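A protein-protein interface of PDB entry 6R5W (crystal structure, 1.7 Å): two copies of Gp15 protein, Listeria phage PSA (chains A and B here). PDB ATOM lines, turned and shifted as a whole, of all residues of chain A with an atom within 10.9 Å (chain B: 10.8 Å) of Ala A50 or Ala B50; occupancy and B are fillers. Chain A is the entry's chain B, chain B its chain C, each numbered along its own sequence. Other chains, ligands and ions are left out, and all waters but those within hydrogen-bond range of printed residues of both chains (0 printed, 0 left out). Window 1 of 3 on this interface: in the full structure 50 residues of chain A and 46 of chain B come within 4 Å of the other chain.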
ATOM      1  N   ALA A  41     -17.042  24.820  10.990  1.00  0.00           N
ATOM      2  CA  ALA A  41     -16.738  23.907  12.081  1.00  0.00           C
ATOM      3  C   ALA A  41     -15.278  23.476  12.051  1.00  0.00           C
ATOM      4  O   ALA A  41     -14.649  23.359  13.099  1.00  0.00           O
ATOM      5  CB  ALA A  41     -17.656  22.670  12.038  1.00  0.00           C
ATOM      6  N   LYS A  42     -14.740  23.205  10.870  1.00  0.00           N
ATOM      7  CA  LYS A  42     -13.362  22.793  10.754  1.00  0.00           C
ATOM      8  C   LYS A  42     -12.421  23.935  11.121  1.00  0.00           C
ATOM      9  O   LYS A  42     -11.396  23.712  11.793  1.00  0.00           O
ATOM     10  CB  LYS A  42     -13.056  22.300   9.341  1.00  0.00           C
ATOM     11  CG  LYS A  42     -13.735  20.987   8.981  1.00  0.00           C
ATOM     12  CD  LYS A  42     -13.492  20.636   7.535  1.00  0.00           C
ATOM     13  CE  LYS A  42     -14.033  19.266   7.233  1.00  0.00           C
ATOM     14  NZ  LYS A  42     -15.494  19.148   7.299  1.00  0.00           N
ATOM     15  N   ALA A  43     -12.742  25.151  10.676  1.00  0.00           N
ATOM     16  CA  ALA A  43     -11.937  26.298  11.056  1.00  0.00           C
ATOM     17  C   ALA A  43     -12.027  26.534  12.568  1.00  0.00           C
ATOM     18  O   ALA A  43     -11.023  26.890  13.210  1.00  0.00           O
ATOM     19  CB  ALA A  43     -12.377  27.544  10.284  1.00  0.00           C
ATOM     20  N   ASP A  44     -13.229  26.415  13.128  1.00  0.00           N
ATOM     21  CA  ASP A  44     -13.422  26.636  14.564  1.00  0.00           C
ATOM     22  C   ASP A  44     -12.583  25.629  15.341  1.00  0.00           C
ATOM     23  O   ASP A  44     -12.011  25.940  16.387  1.00  0.00           O
ATOM     24  CB  ASP A  44     -14.884  26.440  14.963  1.00  0.00           C
ATOM     25  CG  ASP A  44     -15.815  27.526  14.498  1.00  0.00           C
ATOM     26  OD1 ASP A  44     -15.327  28.564  14.033  1.00  0.00           O
ATOM     27  OD2 ASP A  44     -17.052  27.339  14.646  1.00  0.00           O
ATOM     28  N   LYS A  45     -12.557  24.386  14.861  1.00  0.00           N
ATOM     29  CA  LYS A  45     -11.771  23.343  15.515  1.00  0.00           C
ATOM     30  C   LYS A  45     -10.275  23.616  15.431  1.00  0.00           C
ATOM     31  O   LYS A  45      -9.527  23.333  16.395  1.00  0.00           O
ATOM     32  CB  LYS A  45     -12.099  21.991  14.912  1.00  0.00           C
ATOM     33  CG  LYS A  45     -11.297  20.818  15.475  1.00  0.00           C
ATOM     34  CD  LYS A  45     -11.832  20.523  16.883  1.00  0.00           C
ATOM     35  CE  LYS A  45     -11.060  19.389  17.591  1.00  0.00           C
ATOM     36  NZ  LYS A  45     -10.739  18.301  16.621  1.00  0.00           N
ATOM     37  N   ALA A  46      -9.815  24.137  14.296  1.00  0.00           N
ATOM     38  CA  ALA A  46      -8.426  24.522  14.175  1.00  0.00           C
ATOM     39  C   ALA A  46      -8.073  25.609  15.201  1.00  0.00           C
ATOM     40  O   ALA A  46      -6.998  25.566  15.820  1.00  0.00           O
ATOM     41  CB  ALA A  46      -8.103  25.005  12.766  1.00  0.00           C
ATOM     42  N   LEU A  47      -8.952  26.594  15.359  1.00  0.00           N
ATOM     43  CA  LEU A  47      -8.738  27.654  16.330  1.00  0.00           C
ATOM     44  C   LEU A  47      -8.691  27.089  17.747  1.00  0.00           C
ATOM     45  O   LEU A  47      -7.764  27.399  18.515  1.00  0.00           O
ATOM     46  CB  LEU A  47      -9.818  28.726  16.201  1.00  0.00           C
ATOM     47  CG  LEU A  47      -9.777  29.821  17.248  1.00  0.00           C
ATOM     48  CD1 LEU A  47      -8.458  30.560  17.247  1.00  0.00           C
ATOM     49  CD2 LEU A  47     -10.927  30.790  17.040  1.00  0.00           C
ATOM     50  N   ALA A  48      -9.638  26.214  18.084  1.00  0.00           N
ATOM     51  CA  ALA A  48      -9.680  25.634  19.420  1.00  0.00           C
ATOM     52  C   ALA A  48      -8.448  24.789  19.665  1.00  0.00           C
ATOM     53  O   ALA A  48      -7.834  24.874  20.742  1.00  0.00           O
ATOM     54  CB  ALA A  48     -10.929  24.784  19.608  1.00  0.00           C
ATOM     55  N   ASP A  49      -8.022  24.038  18.648  1.00  0.00           N
ATOM     56  CA  ASP A  49      -6.816  23.235  18.760  1.00  0.00           C
ATOM     57  C   ASP A  49      -5.558  24.086  18.941  1.00  0.00           C
ATOM     58  O   ASP A  49      -4.608  23.671  19.655  1.00  0.00           O
ATOM     59  CB  ASP A  49      -6.635  22.371  17.528  1.00  0.00           C
ATOM     60  CG  ASP A  49      -7.599  21.204  17.488  1.00  0.00           C
ATOM     61  OD1 ASP A  49      -8.329  21.034  18.478  1.00  0.00           O
ATOM     62  OD2 ASP A  49      -7.587  20.442  16.488  1.00  0.00           O
ATOM     63  N   ALA A  50      -5.495  25.238  18.247  1.00  0.00           N
ATOM     64  CA  ALA A  50      -4.373  26.165  18.416  1.00  0.00           C
ATOM     65  C   ALA A  50      -4.310  26.683  19.864  1.00  0.00           C
ATOM     66  O   ALA A  50      -3.227  26.707  20.489  1.00  0.00           O
ATOM     67  CB  ALA A  50      -4.511  27.341  17.433  1.00  0.00           C
ATOM     68  N   LYS A  51      -5.463  27.114  20.396  1.00  0.00           N
ATOM     69  CA  LYS A  51      -5.516  27.649  21.755  1.00  0.00           C
ATOM     70  C   LYS A  51      -5.079  26.580  22.772  1.00  0.00           C
ATOM     71  O   LYS A  51      -4.287  26.858  23.686  1.00  0.00           O
ATOM     72  CB  LYS A  51      -6.922  28.114  22.070  1.00  0.00           C
ATOM     73  CG  LYS A  51      -7.392  29.288  21.262  1.00  0.00           C
ATOM     74  CD  LYS A  51      -8.836  29.708  21.704  1.00  0.00           C
ATOM     75  CE  LYS A  51      -9.217  30.951  20.939  1.00  0.00           C
ATOM     76  NZ  LYS A  51     -10.637  31.327  21.216  1.00  0.00           N
ATOM     77  N   ALA A  52      -5.574  25.348  22.604  1.00  0.00           N
ATOM     78  CA  ALA A  52      -5.232  24.236  23.491  1.00  0.00           C
ATOM     79  C   ALA A  52      -3.750  23.923  23.410  1.00  0.00           C
ATOM     80  O   ALA A  52      -3.115  23.616  24.438  1.00  0.00           O
ATOM     81  CB  ALA A  52      -6.075  22.995  23.152  1.00  0.00           C
ATOM     82  N   PHE A  53      -3.190  23.955  22.195  1.00  0.00           N
ATOM     83  CA  PHE A  53      -1.765  23.724  22.009  1.00  0.00           C
ATOM     84  C   PHE A  53      -0.951  24.822  22.706  1.00  0.00           C
ATOM     85  O   PHE A  53       0.051  24.541  23.378  1.00  0.00           O
ATOM     86  CB  PHE A  53      -1.406  23.677  20.531  1.00  0.00           C
ATOM     87  CG  PHE A  53       0.086  23.807  20.247  1.00  0.00           C
ATOM     88  CD1 PHE A  53       0.916  22.711  20.319  1.00  0.00           C
ATOM     89  CD2 PHE A  53       0.626  25.035  19.900  1.00  0.00           C
ATOM     90  CE1 PHE A  53       2.286  22.826  20.057  1.00  0.00           C
ATOM     91  CE2 PHE A  53       2.023  25.186  19.631  1.00  0.00           C
ATOM     92  CZ  PHE A  53       2.845  24.069  19.703  1.00  0.00           C
ATOM     93  N   PHE A  54      -1.364  26.085  22.574  1.00  0.00           N
ATOM     94  CA  PHE A  54      -0.656  27.145  23.286  1.00  0.00           C
ATOM     95  C   PHE A  54      -0.722  26.947  24.811  1.00  0.00           C
ATOM     96  O   PHE A  54       0.279  27.173  25.507  1.00  0.00           O
ATOM     97  CB  PHE A  54      -1.228  28.493  22.888  1.00  0.00           C
ATOM     98  CG  PHE A  54      -0.882  29.586  23.832  1.00  0.00           C
ATOM     99  CD1 PHE A  54       0.381  30.126  23.878  1.00  0.00           C
ATOM    100  CD2 PHE A  54      -1.864  30.101  24.676  1.00  0.00           C
ATOM    101  CE1 PHE A  54       0.673  31.143  24.783  1.00  0.00           C
ATOM    102  CE2 PHE A  54      -1.591  31.110  25.530  1.00  0.00           C
ATOM    103  CZ  PHE A  54      -0.301  31.621  25.602  1.00  0.00           C
ATOM    104  N   GLU A  55      -1.888  26.595  25.350  1.00  0.00           N
ATOM    105  CA  GLU A  55      -2.022  26.473  26.801  1.00  0.00           C
ATOM    106  C   GLU A  55      -1.121  25.362  27.325  1.00  0.00           C
ATOM    107  O   GLU A  55      -0.392  25.533  28.304  1.00  0.00           O
ATOM    108  CB  GLU A  55      -3.460  26.181  27.181  1.00  0.00           C
ATOM    109  CG  GLU A  55      -4.420  27.391  26.985  1.00  0.00           C
ATOM    110  CD  GLU A  55      -4.625  28.286  28.193  1.00  0.00           C
ATOM    111  OE1 GLU A  55      -3.931  28.102  29.227  1.00  0.00           O
ATOM    112  OE2 GLU A  55      -5.524  29.153  28.108  1.00  0.00           O
ATOM    113  N   LEU A  56      -1.096  24.247  26.608  1.00  0.00           N
ATOM    114  CA  LEU A  56      -0.250  23.119  26.938  1.00  0.00           C
ATOM    115  C   LEU A  56       1.212  23.485  26.843  1.00  0.00           C
ATOM    116  O   LEU A  56       1.989  23.142  27.733  1.00  0.00           O
ATOM    117  CB  LEU A  56      -0.584  21.984  25.977  1.00  0.00           C
ATOM    118  CG  LEU A  56      -0.040  20.612  26.311  1.00  0.00           C
ATOM    119  CD1 LEU A  56      -0.672  20.166  27.626  1.00  0.00           C
ATOM    120  CD2 LEU A  56      -0.341  19.701  25.152  1.00  0.00           C
ATOM    121  N   SER A  57       1.623  24.139  25.754  1.00  0.00           N
ATOM    122  CA  SER A  57       3.031  24.418  25.545  1.00  0.00           C
ATOM    123  C   SER A  57       3.577  25.361  26.616  1.00  0.00           C
ATOM    124  O   SER A  57       4.770  25.368  26.898  1.00  0.00           O
ATOM    125  CB  SER A  57       3.277  25.069  24.182  1.00  0.00           C
ATOM    126  OG  SER A  57       2.996  24.196  23.123  1.00  0.00           O
ATOM    127  N   SER A  58       2.722  26.183  27.189  1.00  0.00           N
ATOM    128  CA  SER A  58       3.170  27.186  28.152  1.00  0.00           C
ATOM    129  C   SER A  58       2.802  26.855  29.604  1.00  0.00           C
ATOM    130  O   SER A  58       2.938  27.704  30.465  1.00  0.00           O
ATOM    131  CB  SER A  58       2.641  28.549  27.680  1.00  0.00           C
ATOM    132  OG  SER A  58       1.220  28.586  27.703  1.00  0.00           O
ATOM    133  N   ALA B  41     -11.139  31.687   3.491  1.00  0.00           N
ATOM    134  CA  ALA B  41     -11.371  32.843   4.348  1.00  0.00           C
ATOM    135  C   ALA B  41     -11.611  32.402   5.799  1.00  0.00           C
ATOM    136  O   ALA B  41     -11.135  33.051   6.751  1.00  0.00           O
ATOM    137  CB  ALA B  41     -12.547  33.687   3.819  1.00  0.00           C
ATOM    138  N   LYS B  42     -12.356  31.325   5.982  1.00  0.00           N
ATOM    139  CA  LYS B  42     -12.635  30.820   7.322  1.00  0.00           C
ATOM    140  C   LYS B  42     -11.353  30.321   7.982  1.00  0.00           C
ATOM    141  O   LYS B  42     -11.163  30.545   9.174  1.00  0.00           O
ATOM    142  CB  LYS B  42     -13.708  29.721   7.257  1.00  0.00           C
ATOM    143  CG  LYS B  42     -15.129  30.264   6.861  1.00  0.00           C
ATOM    144  CD  LYS B  42     -16.140  29.083   6.665  1.00  0.00           C
ATOM    145  CE  LYS B  42     -17.543  29.608   6.484  1.00  0.00           C
ATOM    146  NZ  LYS B  42     -17.606  30.383   5.168  1.00  0.00           N
ATOM    147  N   ALA B  43     -10.476  29.664   7.226  1.00  0.00           N
ATOM    148  CA  ALA B  43      -9.192  29.213   7.752  1.00  0.00           C
ATOM    149  C   ALA B  43      -8.278  30.391   8.082  1.00  0.00           C
ATOM    150  O   ALA B  43      -7.614  30.389   9.129  1.00  0.00           O
ATOM    151  CB  ALA B  43      -8.496  28.276   6.767  1.00  0.00           C
ATOM    152  N   ASP B  44      -8.264  31.395   7.204  1.00  0.00           N
ATOM    153  CA  ASP B  44      -7.466  32.584   7.414  1.00  0.00           C
ATOM    154  C   ASP B  44      -7.899  33.297   8.689  1.00  0.00           C
ATOM    155  O   ASP B  44      -7.047  33.791   9.436  1.00  0.00           O
ATOM    156  CB  ASP B  44      -7.589  33.559   6.251  1.00  0.00           C
ATOM    157  CG  ASP B  44      -6.856  33.101   4.973  1.00  0.00           C
ATOM    158  OD1 ASP B  44      -6.086  32.122   4.997  1.00  0.00           O
ATOM    159  OD2 ASP B  44      -7.070  33.772   3.950  1.00  0.00           O
ATOM    160  N   LYS B  45      -9.219  33.389   8.929  1.00  0.00           N
ATOM    161  CA  LYS B  45      -9.740  34.008  10.135  1.00  0.00           C
ATOM    162  C   LYS B  45      -9.397  33.183  11.396  1.00  0.00           C
ATOM    163  O   LYS B  45      -9.063  33.755  12.440  1.00  0.00           O
ATOM    164  CB  LYS B  45     -11.244  34.195  10.029  1.00  0.00           C
ATOM    165  CG  LYS B  45     -11.873  34.728  11.297  1.00  0.00           C
ATOM    166  CD  LYS B  45     -13.292  35.303  11.051  1.00  0.00           C
ATOM    167  CE  LYS B  45     -13.824  36.052  12.268  1.00  0.00           C
ATOM    168  NZ  LYS B  45     -13.763  35.251  13.546  1.00  0.00           N
ATOM    169  N   ALA B  46      -9.434  31.849  11.312  1.00  0.00           N
ATOM    170  CA  ALA B  46      -8.995  31.036  12.433  1.00  0.00           C
ATOM    171  C   ALA B  46      -7.532  31.324  12.789  1.00  0.00           C
ATOM    172  O   ALA B  46      -7.183  31.445  13.983  1.00  0.00           O
ATOM    173  CB  ALA B  46      -9.156  29.547  12.134  1.00  0.00           C
ATOM    174  N   LEU B  47      -6.664  31.461  11.770  1.00  0.00           N
ATOM    175  CA  LEU B  47      -5.258  31.800  12.015  1.00  0.00           C
ATOM    176  C   LEU B  47      -5.126  33.175  12.655  1.00  0.00           C
ATOM    177  O   LEU B  47      -4.397  33.341  13.662  1.00  0.00           O
ATOM    178  CB  LEU B  47      -4.457  31.743  10.707  1.00  0.00           C
ATOM    179  CG  LEU B  47      -3.005  32.206  10.794  1.00  0.00           C
ATOM    180  CD1 LEU B  47      -2.263  31.355  11.814  1.00  0.00           C
ATOM    181  CD2 LEU B  47      -2.321  32.178   9.433  1.00  0.00           C
ATOM    182  N   ALA B  48      -5.861  34.159  12.114  1.00  0.00           N
ATOM    183  CA  ALA B  48      -5.762  35.509  12.653  1.00  0.00           C
ATOM    184  C   ALA B  48      -6.280  35.557  14.086  1.00  0.00           C
ATOM    185  O   ALA B  48      -5.711  36.266  14.950  1.00  0.00           O
ATOM    186  CB  ALA B  48      -6.509  36.498  11.795  1.00  0.00           C
ATOM    187  N   ASP B  49      -7.371  34.839  14.364  1.00  0.00           N
ATOM    188  CA  ASP B  49      -7.914  34.789  15.725  1.00  0.00           C
ATOM    189  C   ASP B  49      -6.938  34.113  16.700  1.00  0.00           C
ATOM    190  O   ASP B  49      -6.806  34.532  17.865  1.00  0.00           O
ATOM    191  CB  ASP B  49      -9.219  34.035  15.715  1.00  0.00           C
ATOM    192  CG  ASP B  49     -10.403  34.832  15.071  1.00  0.00           C
ATOM    193  OD1 ASP B  49     -10.249  36.041  14.843  1.00  0.00           O
ATOM    194  OD2 ASP B  49     -11.475  34.207  14.785  1.00  0.00           O
ATOM    195  N   ALA B  50      -6.270  33.038  16.258  1.00  0.00           N
ATOM    196  CA  ALA B  50      -5.280  32.361  17.093  1.00  0.00           C
ATOM    197  C   ALA B  50      -4.129  33.293  17.466  1.00  0.00           C
ATOM    198  O   ALA B  50      -3.662  33.332  18.619  1.00  0.00           O
ATOM    199  CB  ALA B  50      -4.731  31.150  16.342  1.00  0.00           C
ATOM    200  N   LYS B  51      -3.625  34.020  16.485  1.00  0.00           N
ATOM    201  CA  LYS B  51      -2.519  34.943  16.726  1.00  0.00           C
ATOM    202  C   LYS B  51      -2.928  36.029  17.726  1.00  0.00           C
ATOM    203  O   LYS B  51      -2.171  36.356  18.635  1.00  0.00           O
ATOM    204  CB  LYS B  51      -2.075  35.590  15.424  1.00  0.00           C
ATOM    205  CG  LYS B  51      -1.348  34.617  14.452  1.00  0.00           C
ATOM    206  CD  LYS B  51      -1.009  35.384  13.175  1.00  0.00           C
ATOM    207  CE  LYS B  51      -0.200  34.526  12.177  1.00  0.00           C
ATOM    208  NZ  LYS B  51      -0.073  35.283  10.890  1.00  0.00           N
ATOM    209  N   ALA B  52      -4.129  36.585  17.560  1.00  0.00           N
ATOM    210  CA  ALA B  52      -4.632  37.604  18.467  1.00  0.00           C
ATOM    211  C   ALA B  52      -4.781  37.037  19.875  1.00  0.00           C
ATOM    212  O   ALA B  52      -4.462  37.710  20.860  1.00  0.00           O
ATOM    213  CB  ALA B  52      -5.969  38.148  17.963  1.00  0.00           C
ATOM    214  N   PHE B  53      -5.274  35.804  19.987  1.00  0.00           N
ATOM    215  CA  PHE B  53      -5.449  35.209  21.302  1.00  0.00           C
ATOM    216  C   PHE B  53      -4.104  34.974  21.982  1.00  0.00           C
ATOM    217  O   PHE B  53      -3.927  35.231  23.182  1.00  0.00           O
ATOM    218  CB  PHE B  53      -6.192  33.909  21.151  1.00  0.00           C
ATOM    219  CG  PHE B  53      -6.240  33.092  22.423  1.00  0.00           C
ATOM    220  CD1 PHE B  53      -7.180  33.372  23.375  1.00  0.00           C
ATOM    221  CD2 PHE B  53      -5.328  32.089  22.635  1.00  0.00           C
ATOM    222  CE1 PHE B  53      -7.229  32.601  24.546  1.00  0.00           C
ATOM    223  CE2 PHE B  53      -5.368  31.330  23.797  1.00  0.00           C
ATOM    224  CZ  PHE B  53      -6.332  31.589  24.717  1.00  0.00           C
ATOM    225  N   PHE B  54      -3.135  34.492  21.225  1.00  0.00           N
ATOM    226  CA  PHE B  54      -1.815  34.239  21.798  1.00  0.00           C
ATOM    227  C   PHE B  54      -1.170  35.531  22.281  1.00  0.00           C
ATOM    228  O   PHE B  54      -0.627  35.599  23.386  1.00  0.00           O
ATOM    229  CB  PHE B  54      -0.920  33.567  20.757  1.00  0.00           C
ATOM    230  CG  PHE B  54       0.482  33.631  21.109  1.00  0.00           C
ATOM    231  CD1 PHE B  54       0.969  32.855  22.142  1.00  0.00           C
ATOM    232  CD2 PHE B  54       1.336  34.519  20.474  1.00  0.00           C
ATOM    233  CE1 PHE B  54       2.313  32.957  22.505  1.00  0.00           C
ATOM    234  CE2 PHE B  54       2.655  34.584  20.841  1.00  0.00           C
ATOM    235  CZ  PHE B  54       3.115  33.823  21.857  1.00  0.00           C
ATOM    236  N   GLU B  55      -1.225  36.569  21.455  1.00  0.00           N
ATOM    237  CA  GLU B  55      -0.556  37.829  21.800  1.00  0.00           C
ATOM    238  C   GLU B  55      -1.188  38.469  23.049  1.00  0.00           C
ATOM    239  O   GLU B  55      -0.470  38.986  23.926  1.00  0.00           O
ATOM    240  CB  GLU B  55      -0.647  38.808  20.630  1.00  0.00           C
ATOM    241  CG  GLU B  55       0.343  38.536  19.522  1.00  0.00           C
ATOM    242  CD  GLU B  55       0.261  39.615  18.436  1.00  0.00           C
ATOM    243  OE1 GLU B  55       0.693  39.335  17.295  1.00  0.00           O
ATOM    244  OE2 GLU B  55      -0.252  40.736  18.717  1.00  0.00           O
ATOM    245  N   LEU B  56      -2.515  38.435  23.141  1.00  0.00           N
ATOM    246  CA  LEU B  56      -3.185  38.917  24.361  1.00  0.00           C
ATOM    247  C   LEU B  56      -2.864  38.040  25.580  1.00  0.00           C
ATOM    248  O   LEU B  56      -2.553  38.545  26.661  1.00  0.00           O
ATOM    249  CB  LEU B  56      -4.694  38.975  24.142  1.00  0.00           C
ATOM    250  CG  LEU B  56      -5.441  39.572  25.347  1.00  0.00           C
ATOM    251  CD1 LEU B  56      -4.969  40.962  25.611  1.00  0.00           C
ATOM    252  CD2 LEU B  56      -6.909  39.537  25.084  1.00  0.00           C
ATOM    253  N   SER B  57      -2.942  36.720  25.410  1.00  0.00           N
ATOM    254  CA  SER B  57      -2.746  35.772  26.503  1.00  0.00           C
ATOM    255  C   SER B  57      -1.362  35.891  27.128  1.00  0.00           C
ATOM    256  O   SER B  57      -1.208  35.703  28.351  1.00  0.00           O
ATOM    257  CB  SER B  57      -2.938  34.348  25.988  1.00  0.00           C
ATOM    258  OG  SER B  57      -4.284  34.123  25.661  1.00  0.00           O
ATOM    259  N   SER B  58      -0.349  36.205  26.316  1.00  0.00           N
ATOM    260  CA  SER B  58       1.025  36.238  26.799  1.00  0.00           C
ATOM    261  C   SER B  58       1.481  37.655  27.152  1.00  0.00           C
ATOM    262  O   SER B  58       2.655  37.860  27.418  1.00  0.00           O
ATOM    263  CB  SER B  58       1.942  35.589  25.732  1.00  0.00           C
ATOM    264  OG  SER B  58       2.040  36.424  24.562  1.00  0.00           O
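Ala A50 touches just one residue of chain B: Ala B50 (3.97 Å). Of chain A, only Leu A47 (3.5 Å) and Ala A50 (3.97 Å) come within 4 Å of Ala B50. No residue of chain B comes within 4 Å of Ala A46. No residue of chain B comes within 4 Å of Asp A49. Of chain A, only Ala A43 (3.4 Å) and Leu A47 (3.6 Å) come within 4 Å of Ala B46. No residue of chain A comes within 4 Å of Ala B48. Asp B49 touches one residue of chain A. No residue of chain A comes within 4 Å of Ala B52. Of the printed residues of chain A, Phe B53 touches Lys A51 (3.7 Å) and Phe A54 (3.8 Å). Of the printed residues of chain B, Ala A43 touches Lys B42 (3.4 Å) and Ala B46 (3.4 Å). Of the printed residues of chain A, Ser B57 touches Phe A54. Lys B45 touches none of the printed residues of chain A. The nearest residue of chain A that does not touch Ala B50 is Lys A51 (5.6 Å). The nearest printed residue of chain B that does not touch Phe A54 is Ser B58 (4.6 Å).
Leu A47 touches Asp B49, but with the chains exchanged Asp A49 does not touch Leu B47 (10.2 Å). Leu A47 touches Ala B50, but with the chains exchanged Ala A50 does not touch Leu B47 (7.1 Å). Ala A50 touches its own counterpart, Ala B50. Phe A54 touches Phe B53, but with the chains exchanged Phe A53 does not touch Phe B54 (8.1 Å). Positions printed for both chains: 41, 42, 43, 44, 45, 46, 47, 48, 49, 50, 51, 52, 53, 54, 55, 56, 57 and 58.
Among the printed residues, merely in contact across the chains: Phe A54 with Phe B54, Ala A43 with Ala B46, Ala A43 with Lys B42, Leu A47 with Ala B50, Phe A54 with Ser B57, Leu A47 with Ala B46, Lys A51 with Phe B53, Phe A54 with Phe B53, Leu A47 with Asp B49 and Ala A50 with Ala B50.
Of the 18 printed residues of chain A, 5 touch a printed residue of chain B. Printed residues of chain A that touch a printed residue of chain B: Ala A43, Leu A47, Ala A50, Lys A51 and Phe A54. Hydrophobic or aromatic side chains of chain A within 4 Å of the printed part of chain B: Ala A43, Leu A47, Ala A50 and Phe A54. Among the printed residues, 10 pairs touch across the chains. Among the printed residues, no Asp or Glu carboxylate lies within 4 Å of a Lys or Arg side-chain nitrogen of the other chain.
The backbone carbonyl oxygen (O) of Phe A54 lies within hydrogen-bond range of the side-chain hydroxyl (OG) of Ser A58 (2.8 Å). OD2 of Asp B49 is in salt-bridge range of NZ of Lys B45, 2.8 Å away. The backbone carbonyl oxygen (O) of Phe B53 is in hydrogen-bond range of the side-chain hydroxyl (OG) of Ser B57. The side-chain hydroxyl (OG) of Ser B58 is in hydrogen-bond range of the backbone carbonyl oxygen (O) of Phe B54 (3.0 Å).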
